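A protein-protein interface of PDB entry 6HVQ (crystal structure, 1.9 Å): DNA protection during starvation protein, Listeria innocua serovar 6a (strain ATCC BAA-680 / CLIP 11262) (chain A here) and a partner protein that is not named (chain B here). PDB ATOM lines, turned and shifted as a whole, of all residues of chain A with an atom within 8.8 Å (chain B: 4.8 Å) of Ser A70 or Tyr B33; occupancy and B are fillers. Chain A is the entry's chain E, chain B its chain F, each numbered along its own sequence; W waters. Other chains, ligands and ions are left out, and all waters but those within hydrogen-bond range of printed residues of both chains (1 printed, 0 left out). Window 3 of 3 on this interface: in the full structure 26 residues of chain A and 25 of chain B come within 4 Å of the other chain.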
ATOM      1  N   LYS A  10      -9.317  -9.607 -22.191  1.00  0.00           N
ATOM      2  CA  LYS A  10     -10.684 -10.121 -22.249  1.00  0.00           C
ATOM      3  C   LYS A  10     -11.243 -10.054 -23.665  1.00  0.00           C
ATOM      4  O   LYS A  10     -11.834 -11.023 -24.165  1.00  0.00           O
ATOM      5  CB  LYS A  10     -11.585  -9.355 -21.284  1.00  0.00           C
ATOM      6  CG  LYS A  10     -11.321  -9.623 -19.815  1.00  0.00           C
ATOM      7  CD  LYS A  10     -12.324  -8.844 -18.966  1.00  0.00           C
ATOM      8  CE  LYS A  10     -12.076  -9.013 -17.480  1.00  0.00           C
ATOM      9  NZ  LYS A  10     -13.114  -8.295 -16.690  1.00  0.00           N
ATOM     10  N   GLU A  11     -11.068  -8.910 -24.329  1.00  0.00           N
ATOM     11  CA  GLU A  11     -11.583  -8.765 -25.687  1.00  0.00           C
ATOM     12  C   GLU A  11     -10.888  -9.734 -26.637  1.00  0.00           C
ATOM     13  O   GLU A  11     -11.529 -10.319 -27.519  1.00  0.00           O
ATOM     14  CB  GLU A  11     -11.411  -7.319 -26.154  1.00  0.00           C
ATOM     15  CG  GLU A  11     -12.249  -6.310 -25.371  1.00  0.00           C
ATOM     16  CD  GLU A  11     -13.742  -6.499 -25.565  1.00  0.00           C
ATOM     17  OE1 GLU A  11     -14.160  -6.836 -26.694  1.00  0.00           O
ATOM     18  OE2 GLU A  11     -14.497  -6.312 -24.589  1.00  0.00           O
ATOM     19  N   LEU A  13      -9.626 -12.751 -25.886  1.00  0.00           N
ATOM     20  CA  LEU A  13     -10.150 -14.095 -25.664  1.00  0.00           C
ATOM     21  C   LEU A  13     -11.539 -14.250 -26.271  1.00  0.00           C
ATOM     22  O   LEU A  13     -11.820 -15.249 -26.948  1.00  0.00           O
ATOM     23  CB  LEU A  13     -10.173 -14.412 -24.166  1.00  0.00           C
ATOM     24  CG  LEU A  13      -8.820 -14.609 -23.468  1.00  0.00           C
ATOM     25  CD1 LEU A  13      -9.021 -14.908 -21.990  1.00  0.00           C
ATOM     26  CD2 LEU A  13      -8.024 -15.734 -24.108  1.00  0.00           C
ATOM     27  N   ASN A  14     -12.409 -13.251 -26.086  1.00  0.00           N
ATOM     28  CA  ASN A  14     -13.758 -13.363 -26.640  1.00  0.00           C
ATOM     29  C   ASN A  14     -13.719 -13.428 -28.162  1.00  0.00           C
ATOM     30  O   ASN A  14     -14.441 -14.227 -28.788  1.00  0.00           O
ATOM     31  CB  ASN A  14     -14.613 -12.187 -26.163  1.00  0.00           C
ATOM     32  CG  ASN A  14     -16.014 -12.607 -25.765  1.00  0.00           C
ATOM     33  OD1 ASN A  14     -16.382 -13.778 -25.881  1.00  0.00           O
ATOM     34  ND2 ASN A  14     -16.808 -11.651 -25.294  1.00  0.00           N
ATOM     35  N   HIS A  15     -12.844 -12.628 -28.775  1.00  0.00           N
ATOM     36  CA  HIS A  15     -12.660 -12.711 -30.218  1.00  0.00           C
ATOM     37  C   HIS A  15     -12.308 -14.130 -30.640  1.00  0.00           C
ATOM     38  O   HIS A  15     -12.807 -14.627 -31.661  1.00  0.00           O
ATOM     39  CB  HIS A  15     -11.565 -11.746 -30.671  1.00  0.00           C
ATOM     40  CG  HIS A  15     -11.418 -11.674 -32.156  1.00  0.00           C
ATOM     41  ND1 HIS A  15     -12.282 -10.955 -32.953  1.00  0.00           N
ATOM     42  CD2 HIS A  15     -10.535 -12.266 -32.995  1.00  0.00           C
ATOM     43  CE1 HIS A  15     -11.925 -11.091 -34.218  1.00  0.00           C
ATOM     44  NE2 HIS A  15     -10.868 -11.881 -34.270  1.00  0.00           N
ATOM     45  N   VAL A  17     -13.115 -16.922 -29.012  1.00  0.00           N
ATOM     46  CA  VAL A  17     -14.311 -17.759 -28.902  1.00  0.00           C
ATOM     47  C   VAL A  17     -15.100 -17.705 -30.209  1.00  0.00           C
ATOM     48  O   VAL A  17     -15.477 -18.744 -30.786  1.00  0.00           O
ATOM     49  CB  VAL A  17     -15.169 -17.325 -27.697  1.00  0.00           C
ATOM     50  CG1 VAL A  17     -16.465 -18.121 -27.642  1.00  0.00           C
ATOM     51  CG2 VAL A  17     -14.383 -17.478 -26.399  1.00  0.00           C
ATOM     52  N   VAL A  60     -10.798 -21.492 -23.742  1.00  0.00           N
ATOM     53  CA  VAL A  60     -10.688 -20.039 -23.882  1.00  0.00           C
ATOM     54  C   VAL A  60     -11.880 -19.354 -23.223  1.00  0.00           C
ATOM     55  O   VAL A  60     -11.724 -18.381 -22.476  1.00  0.00           O
ATOM     56  CB  VAL A  60     -10.555 -19.652 -25.368  1.00  0.00           C
ATOM     57  CG1 VAL A  60     -10.748 -18.157 -25.574  1.00  0.00           C
ATOM     58  CG2 VAL A  60      -9.191 -20.073 -25.901  1.00  0.00           C
ATOM     59  N   ALA A  61     -13.091 -19.846 -23.497  1.00  0.00           N
ATOM     60  CA  ALA A  61     -14.279 -19.241 -22.900  1.00  0.00           C
ATOM     61  C   ALA A  61     -14.226 -19.298 -21.376  1.00  0.00           C
ATOM     62  O   ALA A  61     -14.616 -18.340 -20.695  1.00  0.00           O
ATOM     63  CB  ALA A  61     -15.531 -19.940 -23.421  1.00  0.00           C
ATOM     64  N   GLU A  62     -13.739 -20.411 -20.822  1.00  0.00           N
ATOM     65  CA  GLU A  62     -13.741 -20.572 -19.371  1.00  0.00           C
ATOM     66  C   GLU A  62     -12.574 -19.843 -18.703  1.00  0.00           C
ATOM     67  O   GLU A  62     -12.691 -19.438 -17.535  1.00  0.00           O
ATOM     68  CB  GLU A  62     -13.782 -22.070 -19.040  1.00  0.00           C
ATOM     69  CG  GLU A  62     -15.215 -22.590 -19.148  1.00  0.00           C
ATOM     70  CD  GLU A  62     -15.357 -24.094 -19.169  1.00  0.00           C
ATOM     71  OE1 GLU A  62     -14.350 -24.828 -19.272  1.00  0.00           O
ATOM     72  OE2 GLU A  62     -16.508 -24.542 -19.021  1.00  0.00           O
ATOM     73  N   ARG A  63     -11.455 -19.642 -19.413  1.00  0.00           N
ATOM     74  CA  ARG A  63     -10.446 -18.714 -18.911  1.00  0.00           C
ATOM     75  C   ARG A  63     -10.997 -17.294 -18.895  1.00  0.00           C
ATOM     76  O   ARG A  63     -10.739 -16.528 -17.958  1.00  0.00           O
ATOM     77  CB  ARG A  63      -9.167 -18.790 -19.752  1.00  0.00           C
ATOM     78  CG  ARG A  63      -8.040 -17.840 -19.300  1.00  0.00           C
ATOM     79  CD  ARG A  63      -7.558 -18.121 -17.881  1.00  0.00           C
ATOM     80  NE  ARG A  63      -6.679 -17.062 -17.380  1.00  0.00           N
ATOM     81  CZ  ARG A  63      -6.378 -16.879 -16.104  1.00  0.00           C
ATOM     82  NH1 ARG A  63      -6.878 -17.689 -15.181  1.00  0.00           N
ATOM     83  NH2 ARG A  63      -5.564 -15.887 -15.743  1.00  0.00           N
ATOM     84  N   LEU A  64     -11.744 -16.921 -19.935  1.00  0.00           N
ATOM     85  CA  LEU A  64     -12.392 -15.616 -19.943  1.00  0.00           C
ATOM     86  C   LEU A  64     -13.316 -15.461 -18.742  1.00  0.00           C
ATOM     87  O   LEU A  64     -13.310 -14.416 -18.078  1.00  0.00           O
ATOM     88  CB  LEU A  64     -13.161 -15.430 -21.254  1.00  0.00           C
ATOM     89  CG  LEU A  64     -13.927 -14.118 -21.432  1.00  0.00           C
ATOM     90  CD1 LEU A  64     -13.012 -12.920 -21.256  1.00  0.00           C
ATOM     91  CD2 LEU A  64     -14.600 -14.102 -22.794  1.00  0.00           C
ATOM     92  N   LEU A  65     -14.110 -16.495 -18.438  1.00  0.00           N
ATOM     93  CA  LEU A  65     -14.949 -16.449 -17.242  1.00  0.00           C
ATOM     94  C   LEU A  65     -14.108 -16.260 -15.987  1.00  0.00           C
ATOM     95  O   LEU A  65     -14.455 -15.461 -15.107  1.00  0.00           O
ATOM     96  CB  LEU A  65     -15.778 -17.729 -17.127  1.00  0.00           C
ATOM     97  CG  LEU A  65     -16.928 -17.909 -18.116  1.00  0.00           C
ATOM     98  CD1 LEU A  65     -17.387 -19.358 -18.114  1.00  0.00           C
ATOM     99  CD2 LEU A  65     -18.085 -16.986 -17.768  1.00  0.00           C
ATOM    100  N   ALA A  66     -12.994 -16.989 -15.892  1.00  0.00           N
ATOM    101  CA  ALA A  66     -12.202 -17.009 -14.671  1.00  0.00           C
ATOM    102  C   ALA A  66     -11.513 -15.680 -14.392  1.00  0.00           C
ATOM    103  O   ALA A  66     -11.151 -15.417 -13.237  1.00  0.00           O
ATOM    104  CB  ALA A  66     -11.160 -18.130 -14.760  1.00  0.00           C
ATOM    105  N   ILE A  67     -11.319 -14.839 -15.408  1.00  0.00           N
ATOM    106  CA  ILE A  67     -10.747 -13.514 -15.206  1.00  0.00           C
ATOM    107  C   ILE A  67     -11.818 -12.427 -15.172  1.00  0.00           C
ATOM    108  O   ILE A  67     -11.491 -11.238 -15.231  1.00  0.00           O
ATOM    109  CB  ILE A  67      -9.674 -13.203 -16.262  1.00  0.00           C
ATOM    110  CG1 ILE A  67     -10.274 -13.214 -17.672  1.00  0.00           C
ATOM    111  CG2 ILE A  67      -8.515 -14.202 -16.145  1.00  0.00           C
ATOM    112  CD1 ILE A  67      -9.309 -12.773 -18.752  1.00  0.00           C
ATOM    113  N   GLY A  68     -13.089 -12.806 -15.077  1.00  0.00           N
ATOM    114  CA  GLY A  68     -14.166 -11.853 -14.896  1.00  0.00           C
ATOM    115  C   GLY A  68     -14.892 -11.431 -16.155  1.00  0.00           C
ATOM    116  O   GLY A  68     -15.644 -10.450 -16.109  1.00  0.00           O
ATOM    117  N   GLY A  69     -14.701 -12.137 -17.273  1.00  0.00           N
ATOM    118  CA  GLY A  69     -15.318 -11.774 -18.529  1.00  0.00           C
ATOM    119  C   GLY A  69     -16.581 -12.573 -18.826  1.00  0.00           C
ATOM    120  O   GLY A  69     -17.028 -13.415 -18.051  1.00  0.00           O
ATOM    121  N   SER A  70     -17.146 -12.296 -19.996  1.00  0.00           N
ATOM    122  CA  SER A  70     -18.418 -12.879 -20.423  1.00  0.00           C
ATOM    123  C   SER A  70     -18.300 -13.347 -21.870  1.00  0.00           C
ATOM    124  O   SER A  70     -18.332 -12.507 -22.793  1.00  0.00           O
ATOM    125  CB  SER A  70     -19.543 -11.857 -20.283  1.00  0.00           C
ATOM    126  OG  SER A  70     -19.674 -11.415 -18.945  1.00  0.00           O
ATOM    127  N   PRO A  71     -18.189 -14.649 -22.127  1.00  0.00           N
ATOM    128  CA  PRO A  71     -17.971 -15.099 -23.505  1.00  0.00           C
ATOM    129  C   PRO A  71     -19.211 -14.947 -24.372  1.00  0.00           C
ATOM    130  O   PRO A  71     -20.344 -15.150 -23.924  1.00  0.00           O
ATOM    131  CB  PRO A  71     -17.588 -16.576 -23.341  1.00  0.00           C
ATOM    132  CG  PRO A  71     -18.204 -16.984 -22.067  1.00  0.00           C
ATOM    133  CD  PRO A  71     -18.132 -15.773 -21.174  1.00  0.00           C
ATOM    134  N   PHE A  72     -18.980 -14.580 -25.631  1.00  0.00           N
ATOM    135  CA  PHE A  72     -20.012 -14.718 -26.645  1.00  0.00           C
ATOM    136  C   PHE A  72     -20.577 -16.130 -26.575  1.00  0.00           C
ATOM    137  O   PHE A  72     -19.852 -17.084 -26.287  1.00  0.00           O
ATOM    138  CB  PHE A  72     -19.429 -14.461 -28.037  1.00  0.00           C
ATOM    139  CG  PHE A  72     -18.831 -13.087 -28.224  1.00  0.00           C
ATOM    140  CD1 PHE A  72     -19.518 -11.943 -27.858  1.00  0.00           C
ATOM    141  CD2 PHE A  72     -17.578 -12.950 -28.791  1.00  0.00           C
ATOM    142  CE1 PHE A  72     -18.957 -10.687 -28.050  1.00  0.00           C
ATOM    143  CE2 PHE A  72     -17.012 -11.705 -28.987  1.00  0.00           C
ATOM    144  CZ  PHE A  72     -17.699 -10.572 -28.618  1.00  0.00           C
ATOM    145  N   SER A  73     -21.892 -16.263 -26.804  1.00  0.00           N
ATOM    146  CA  SER A  73     -22.525 -17.570 -26.665  1.00  0.00           C
ATOM    147  C   SER A  73     -23.759 -17.705 -27.545  1.00  0.00           C
ATOM    148  O   SER A  73     -24.694 -18.435 -27.193  1.00  0.00           O
ATOM    149  CB  SER A  73     -22.905 -17.835 -25.211  1.00  0.00           C
ATOM    150  OG  SER A  73     -23.855 -16.891 -24.761  1.00  0.00           O
ATOM    151  N   THR A  74     -23.767 -17.025 -28.689  1.00  0.00           N
ATOM    152  CA  THR A  74     -24.805 -17.155 -29.704  1.00  0.00           C
ATOM    153  C   THR A  74     -24.134 -17.120 -31.068  1.00  0.00           C
ATOM    154  O   THR A  74     -23.056 -16.539 -31.230  1.00  0.00           O
ATOM    155  CB  THR A  74     -25.853 -16.026 -29.653  1.00  0.00           C
ATOM    156  OG1 THR A  74     -25.206 -14.763 -29.830  1.00  0.00           O
ATOM    157  CG2 THR A  74     -26.635 -16.021 -28.347  1.00  0.00           C
ATOM    158  N   GLU A  77     -23.584 -13.505 -32.264  1.00  0.00           N
ATOM    159  CA  GLU A  77     -22.368 -12.891 -31.738  1.00  0.00           C
ATOM    160  C   GLU A  77     -21.118 -13.426 -32.441  1.00  0.00           C
ATOM    161  O   GLU A  77     -20.210 -12.653 -32.786  1.00  0.00           O
ATOM    162  CB  GLU A  77     -22.288 -13.129 -30.229  1.00  0.00           C
ATOM    163  CG  GLU A  77     -23.276 -12.294 -29.417  1.00  0.00           C
ATOM    164  CD  GLU A  77     -23.309 -12.687 -27.946  1.00  0.00           C
ATOM    165  OE1 GLU A  77     -23.590 -13.867 -27.639  1.00  0.00           O
ATOM    166  OE2 GLU A  77     -23.043 -11.816 -27.096  1.00  0.00           O
ATOM    167  N   GLN B  29     -23.783 -22.133 -23.807  1.00  0.00           N
ATOM    168  CA  GLN B  29     -24.176 -20.944 -23.042  1.00  0.00           C
ATOM    169  C   GLN B  29     -24.585 -21.315 -21.617  1.00  0.00           C
ATOM    170  O   GLN B  29     -24.143 -20.695 -20.636  1.00  0.00           O
ATOM    171  CB  GLN B  29     -25.328 -20.220 -23.753  1.00  0.00           C
ATOM    172  CG  GLN B  29     -25.871 -18.976 -23.033  1.00  0.00           C
ATOM    173  CD  GLN B  29     -27.049 -18.332 -23.765  1.00  0.00           C
ATOM    174  OE1 GLN B  29     -28.207 -18.669 -23.517  1.00  0.00           O
ATOM    175  NE2 GLN B  29     -26.755 -17.407 -24.672  1.00  0.00           N
ATOM    176  N   ILE B  30     -25.455 -22.320 -21.489  1.00  0.00           N
ATOM    177  CA  ILE B  30     -25.919 -22.740 -20.170  1.00  0.00           C
ATOM    178  C   ILE B  30     -24.758 -23.286 -19.349  1.00  0.00           C
ATOM    179  O   ILE B  30     -24.619 -22.983 -18.156  1.00  0.00           O
ATOM    180  CB  ILE B  30     -27.053 -23.773 -20.316  1.00  0.00           C
ATOM    181  CG1 ILE B  30     -28.273 -23.133 -20.998  1.00  0.00           C
ATOM    182  CG2 ILE B  30     -27.422 -24.344 -18.959  1.00  0.00           C
ATOM    183  CD1 ILE B  30     -29.346 -24.129 -21.412  1.00  0.00           C
ATOM    184  N   HIS B  31     -23.927 -24.120 -19.974  1.00  0.00           N
ATOM    185  CA  HIS B  31     -22.742 -24.682 -19.333  1.00  0.00           C
ATOM    186  C   HIS B  31     -21.864 -23.601 -18.710  1.00  0.00           C
ATOM    187  O   HIS B  31     -21.415 -23.726 -17.564  1.00  0.00           O
ATOM    188  CB  HIS B  31     -21.976 -25.477 -20.390  1.00  0.00           C
ATOM    189  CG  HIS B  31     -20.696 -26.094 -19.917  1.00  0.00           C
ATOM    190  ND1 HIS B  31     -20.654 -27.237 -19.151  1.00  0.00           N
ATOM    191  CD2 HIS B  31     -19.406 -25.759 -20.159  1.00  0.00           C
ATOM    192  CE1 HIS B  31     -19.395 -27.570 -18.925  1.00  0.00           C
ATOM    193  NE2 HIS B  31     -18.617 -26.686 -19.523  1.00  0.00           N
ATOM    194  N   TRP B  32     -21.619 -22.523 -19.454  1.00  0.00           N
ATOM    195  CA  TRP B  32     -20.689 -21.484 -19.019  1.00  0.00           C
ATOM    196  C   TRP B  32     -21.300 -20.562 -17.974  1.00  0.00           C
ATOM    197  O   TRP B  32     -20.634 -20.208 -16.995  1.00  0.00           O
ATOM    198  CB  TRP B  32     -20.249 -20.650 -20.222  1.00  0.00           C
ATOM    199  CG  TRP B  32     -19.382 -21.375 -21.189  1.00  0.00           C
ATOM    200  CD1 TRP B  32     -18.555 -22.431 -20.929  1.00  0.00           C
ATOM    201  CD2 TRP B  32     -19.274 -21.116 -22.593  1.00  0.00           C
ATOM    202  NE1 TRP B  32     -17.931 -22.836 -22.088  1.00  0.00           N
ATOM    203  CE2 TRP B  32     -18.357 -22.045 -23.122  1.00  0.00           C
ATOM    204  CE3 TRP B  32     -19.860 -20.182 -23.452  1.00  0.00           C
ATOM    205  CZ2 TRP B  32     -18.016 -22.069 -24.473  1.00  0.00           C
ATOM    206  CZ3 TRP B  32     -19.517 -20.204 -24.791  1.00  0.00           C
ATOM    207  CH2 TRP B  32     -18.608 -21.142 -25.290  1.00  0.00           C
ATOM    208  N   TYR B  33     -22.557 -20.155 -18.161  1.00  0.00           N
ATOM    209  CA  TYR B  33     -23.110 -19.056 -17.379  1.00  0.00           C
ATOM    210  C   TYR B  33     -23.913 -19.491 -16.154  1.00  0.00           C
ATOM    211  O   TYR B  33     -24.271 -18.633 -15.344  1.00  0.00           O
ATOM    212  CB  TYR B  33     -23.991 -18.175 -18.270  1.00  0.00           C
ATOM    213  CG  TYR B  33     -23.214 -17.206 -19.143  1.00  0.00           C
ATOM    214  CD1 TYR B  33     -22.654 -16.056 -18.603  1.00  0.00           C
ATOM    215  CD2 TYR B  33     -23.053 -17.434 -20.503  1.00  0.00           C
ATOM    216  CE1 TYR B  33     -21.950 -15.158 -19.391  1.00  0.00           C
ATOM    217  CE2 TYR B  33     -22.354 -16.540 -21.303  1.00  0.00           C
ATOM    218  CZ  TYR B  33     -21.804 -15.403 -20.738  1.00  0.00           C
ATOM    219  OH  TYR B  33     -21.108 -14.502 -21.514  1.00  0.00           O
ATOM    220  N   MET B  34     -24.191 -20.783 -15.984  1.00  0.00           N
ATOM    221  CA  MET B  34     -25.023 -21.222 -14.867  1.00  0.00           C
ATOM    222  C   MET B  34     -24.372 -20.892 -13.525  1.00  0.00           C
ATOM    223  O   MET B  34     -23.148 -20.929 -13.374  1.00  0.00           O
ATOM    224  CB  MET B  34     -25.278 -22.729 -14.948  1.00  0.00           C
ATOM    225  CG  MET B  34     -23.997 -23.549 -14.960  1.00  0.00           C
ATOM    226  SD  MET B  34     -24.251 -25.304 -14.739  1.00  0.00           S
ATOM    227  CE  MET B  34     -25.362 -25.679 -16.097  1.00  0.00           C
ATOM    228  N   ARG B  35     -25.215 -20.592 -12.536  1.00  0.00           N
ATOM    229  CA  ARG B  35     -24.793 -20.407 -11.155  1.00  0.00           C
ATOM    230  C   ARG B  35     -25.827 -21.040 -10.231  1.00  0.00           C
ATOM    231  O   ARG B  35     -26.991 -21.214 -10.596  1.00  0.00           O
ATOM    232  CB  ARG B  35     -24.635 -18.925 -10.790  1.00  0.00           C
ATOM    233  CG  ARG B  35     -23.560 -18.194 -11.572  1.00  0.00           C
ATOM    234  CD  ARG B  35     -23.464 -16.740 -11.116  1.00  0.00           C
ATOM    235  NE  ARG B  35     -22.485 -15.981 -11.891  1.00  0.00           N
ATOM    236  CZ  ARG B  35     -22.325 -14.665 -11.806  1.00  0.00           C
ATOM    237  NH1 ARG B  35     -23.077 -13.953 -10.981  1.00  0.00           N
ATOM    238  NH2 ARG B  35     -21.410 -14.058 -12.546  1.00  0.00           N
ATOM    239  N   TYR B  89     -26.645 -13.796 -23.483  1.00  0.00           N
ATOM    240  CA  TYR B  89     -26.742 -13.794 -22.025  1.00  0.00           C
ATOM    241  C   TYR B  89     -26.285 -12.428 -21.542  1.00  0.00           C
ATOM    242  O   TYR B  89     -25.088 -12.155 -21.446  1.00  0.00           O
ATOM    243  CB  TYR B  89     -25.906 -14.908 -21.410  1.00  0.00           C
ATOM    244  CG  TYR B  89     -26.225 -15.140 -19.953  1.00  0.00           C
ATOM    245  CD1 TYR B  89     -27.257 -15.986 -19.581  1.00  0.00           C
ATOM    246  CD2 TYR B  89     -25.501 -14.509 -18.945  1.00  0.00           C
ATOM    247  CE1 TYR B  89     -27.562 -16.212 -18.252  1.00  0.00           C
ATOM    248  CE2 TYR B  89     -25.800 -14.728 -17.606  1.00  0.00           C
ATOM    249  CZ  TYR B  89     -26.834 -15.583 -17.271  1.00  0.00           C
ATOM    250  OH  TYR B  89     -27.152 -15.806 -15.952  1.00  0.00           O
ATOM    251  N   LEU B  98     -32.776 -21.255 -16.851  1.00  0.00           N
ATOM    252  CA  LEU B  98     -31.920 -21.865 -17.862  1.00  0.00           C
ATOM    253  C   LEU B  98     -32.424 -23.251 -18.253  1.00  0.00           C
ATOM    254  O   LEU B  98     -32.445 -23.601 -19.440  1.00  0.00           O
ATOM    255  CB  LEU B  98     -30.481 -21.927 -17.346  1.00  0.00           C
ATOM    256  CG  LEU B  98     -29.805 -20.572 -17.103  1.00  0.00           C
ATOM    257  CD1 LEU B  98     -28.426 -20.747 -16.475  1.00  0.00           C
ATOM    258  CD2 LEU B  98     -29.684 -19.771 -18.390  1.00  0.00           C
HETATM  259  O   HOH W   1     -24.046 -14.247 -24.915  1.00  0.00           O
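Among the printed residues, pairs that only touch across the chains: Ala A61 with Trp B32, Glu A62 with Trp B32, Leu A65 with Trp B32, Ser A70 with Tyr B33, Pro A71 with Trp B32, Phe A72 with Trp B32, Ser A73 with Tyr B33 and Thr A74 with Gln B29.
Printed residues of chain B that touch a printed residue of chain A: Gln B29, His B31, Trp B32 and Tyr B33. Printed residues of chain A that touch a printed residue of chain B: Ala A61, Glu A62, Leu A65, Ser A70, Pro A71, Phe A72, Ser A73 and Thr A74. Among the printed residues, 11 pairs touch across the chains. Among the printed residues, no Asp or Glu carboxylate lies within 4 Å of a Lys or Arg side-chain nitrogen of the other chain.
Leu A13 touches none of the printed residues of chain B. Of the printed residues of chain B, Leu A65 touches Trp B32. Ser A70 touches just one residue of chain B: Tyr B33. Of the printed residues of chain A, His B31 touches Glu A62 (3.0 Å). Leu B98 touches none of the printed residues of chain A. The nearest residue of chain A that does not touch Tyr B33 is Leu A65 (4.6 Å). The nearest printed residue of chain B that does not touch Ser A73 is Trp B32 (4.2 Å).
Water W1 lies within hydrogen-bond range of OG of Ser A73 (2.7 Å), OE1 of Glu A77 (2.8 Å) and N of Tyr B89 (3.0 Å).
ND2 of Asn A14 is in hydrogen-bond range of O of Ser A70 (3.1 Å). The backbone NH (N) of Phe A72 is in hydrogen-bond range of the side-chain amide oxygen (OD1) of Asn A14, at 2.7 Å. N of Ser A73 lies within hydrogen-bond range of OE1 of Glu A77. The side-chain hydroxyl (OG1) of Thr A74 is in hydrogen-bond range of the side-chain carboxylate (OE1) of Glu A77 (2.9 Å).
OG of Ser A73 is in hydrogen-bond range of NE2 of Gln B29 (2.9 Å). The backbone carbonyl oxygen (O) of Pro A71 sits at hydrogen-bond distance from the side-chain hydroxyl (OH) of Tyr B33. NE2 of His B31 lies close to OE2 of Glu A62, 3.0 Å away.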
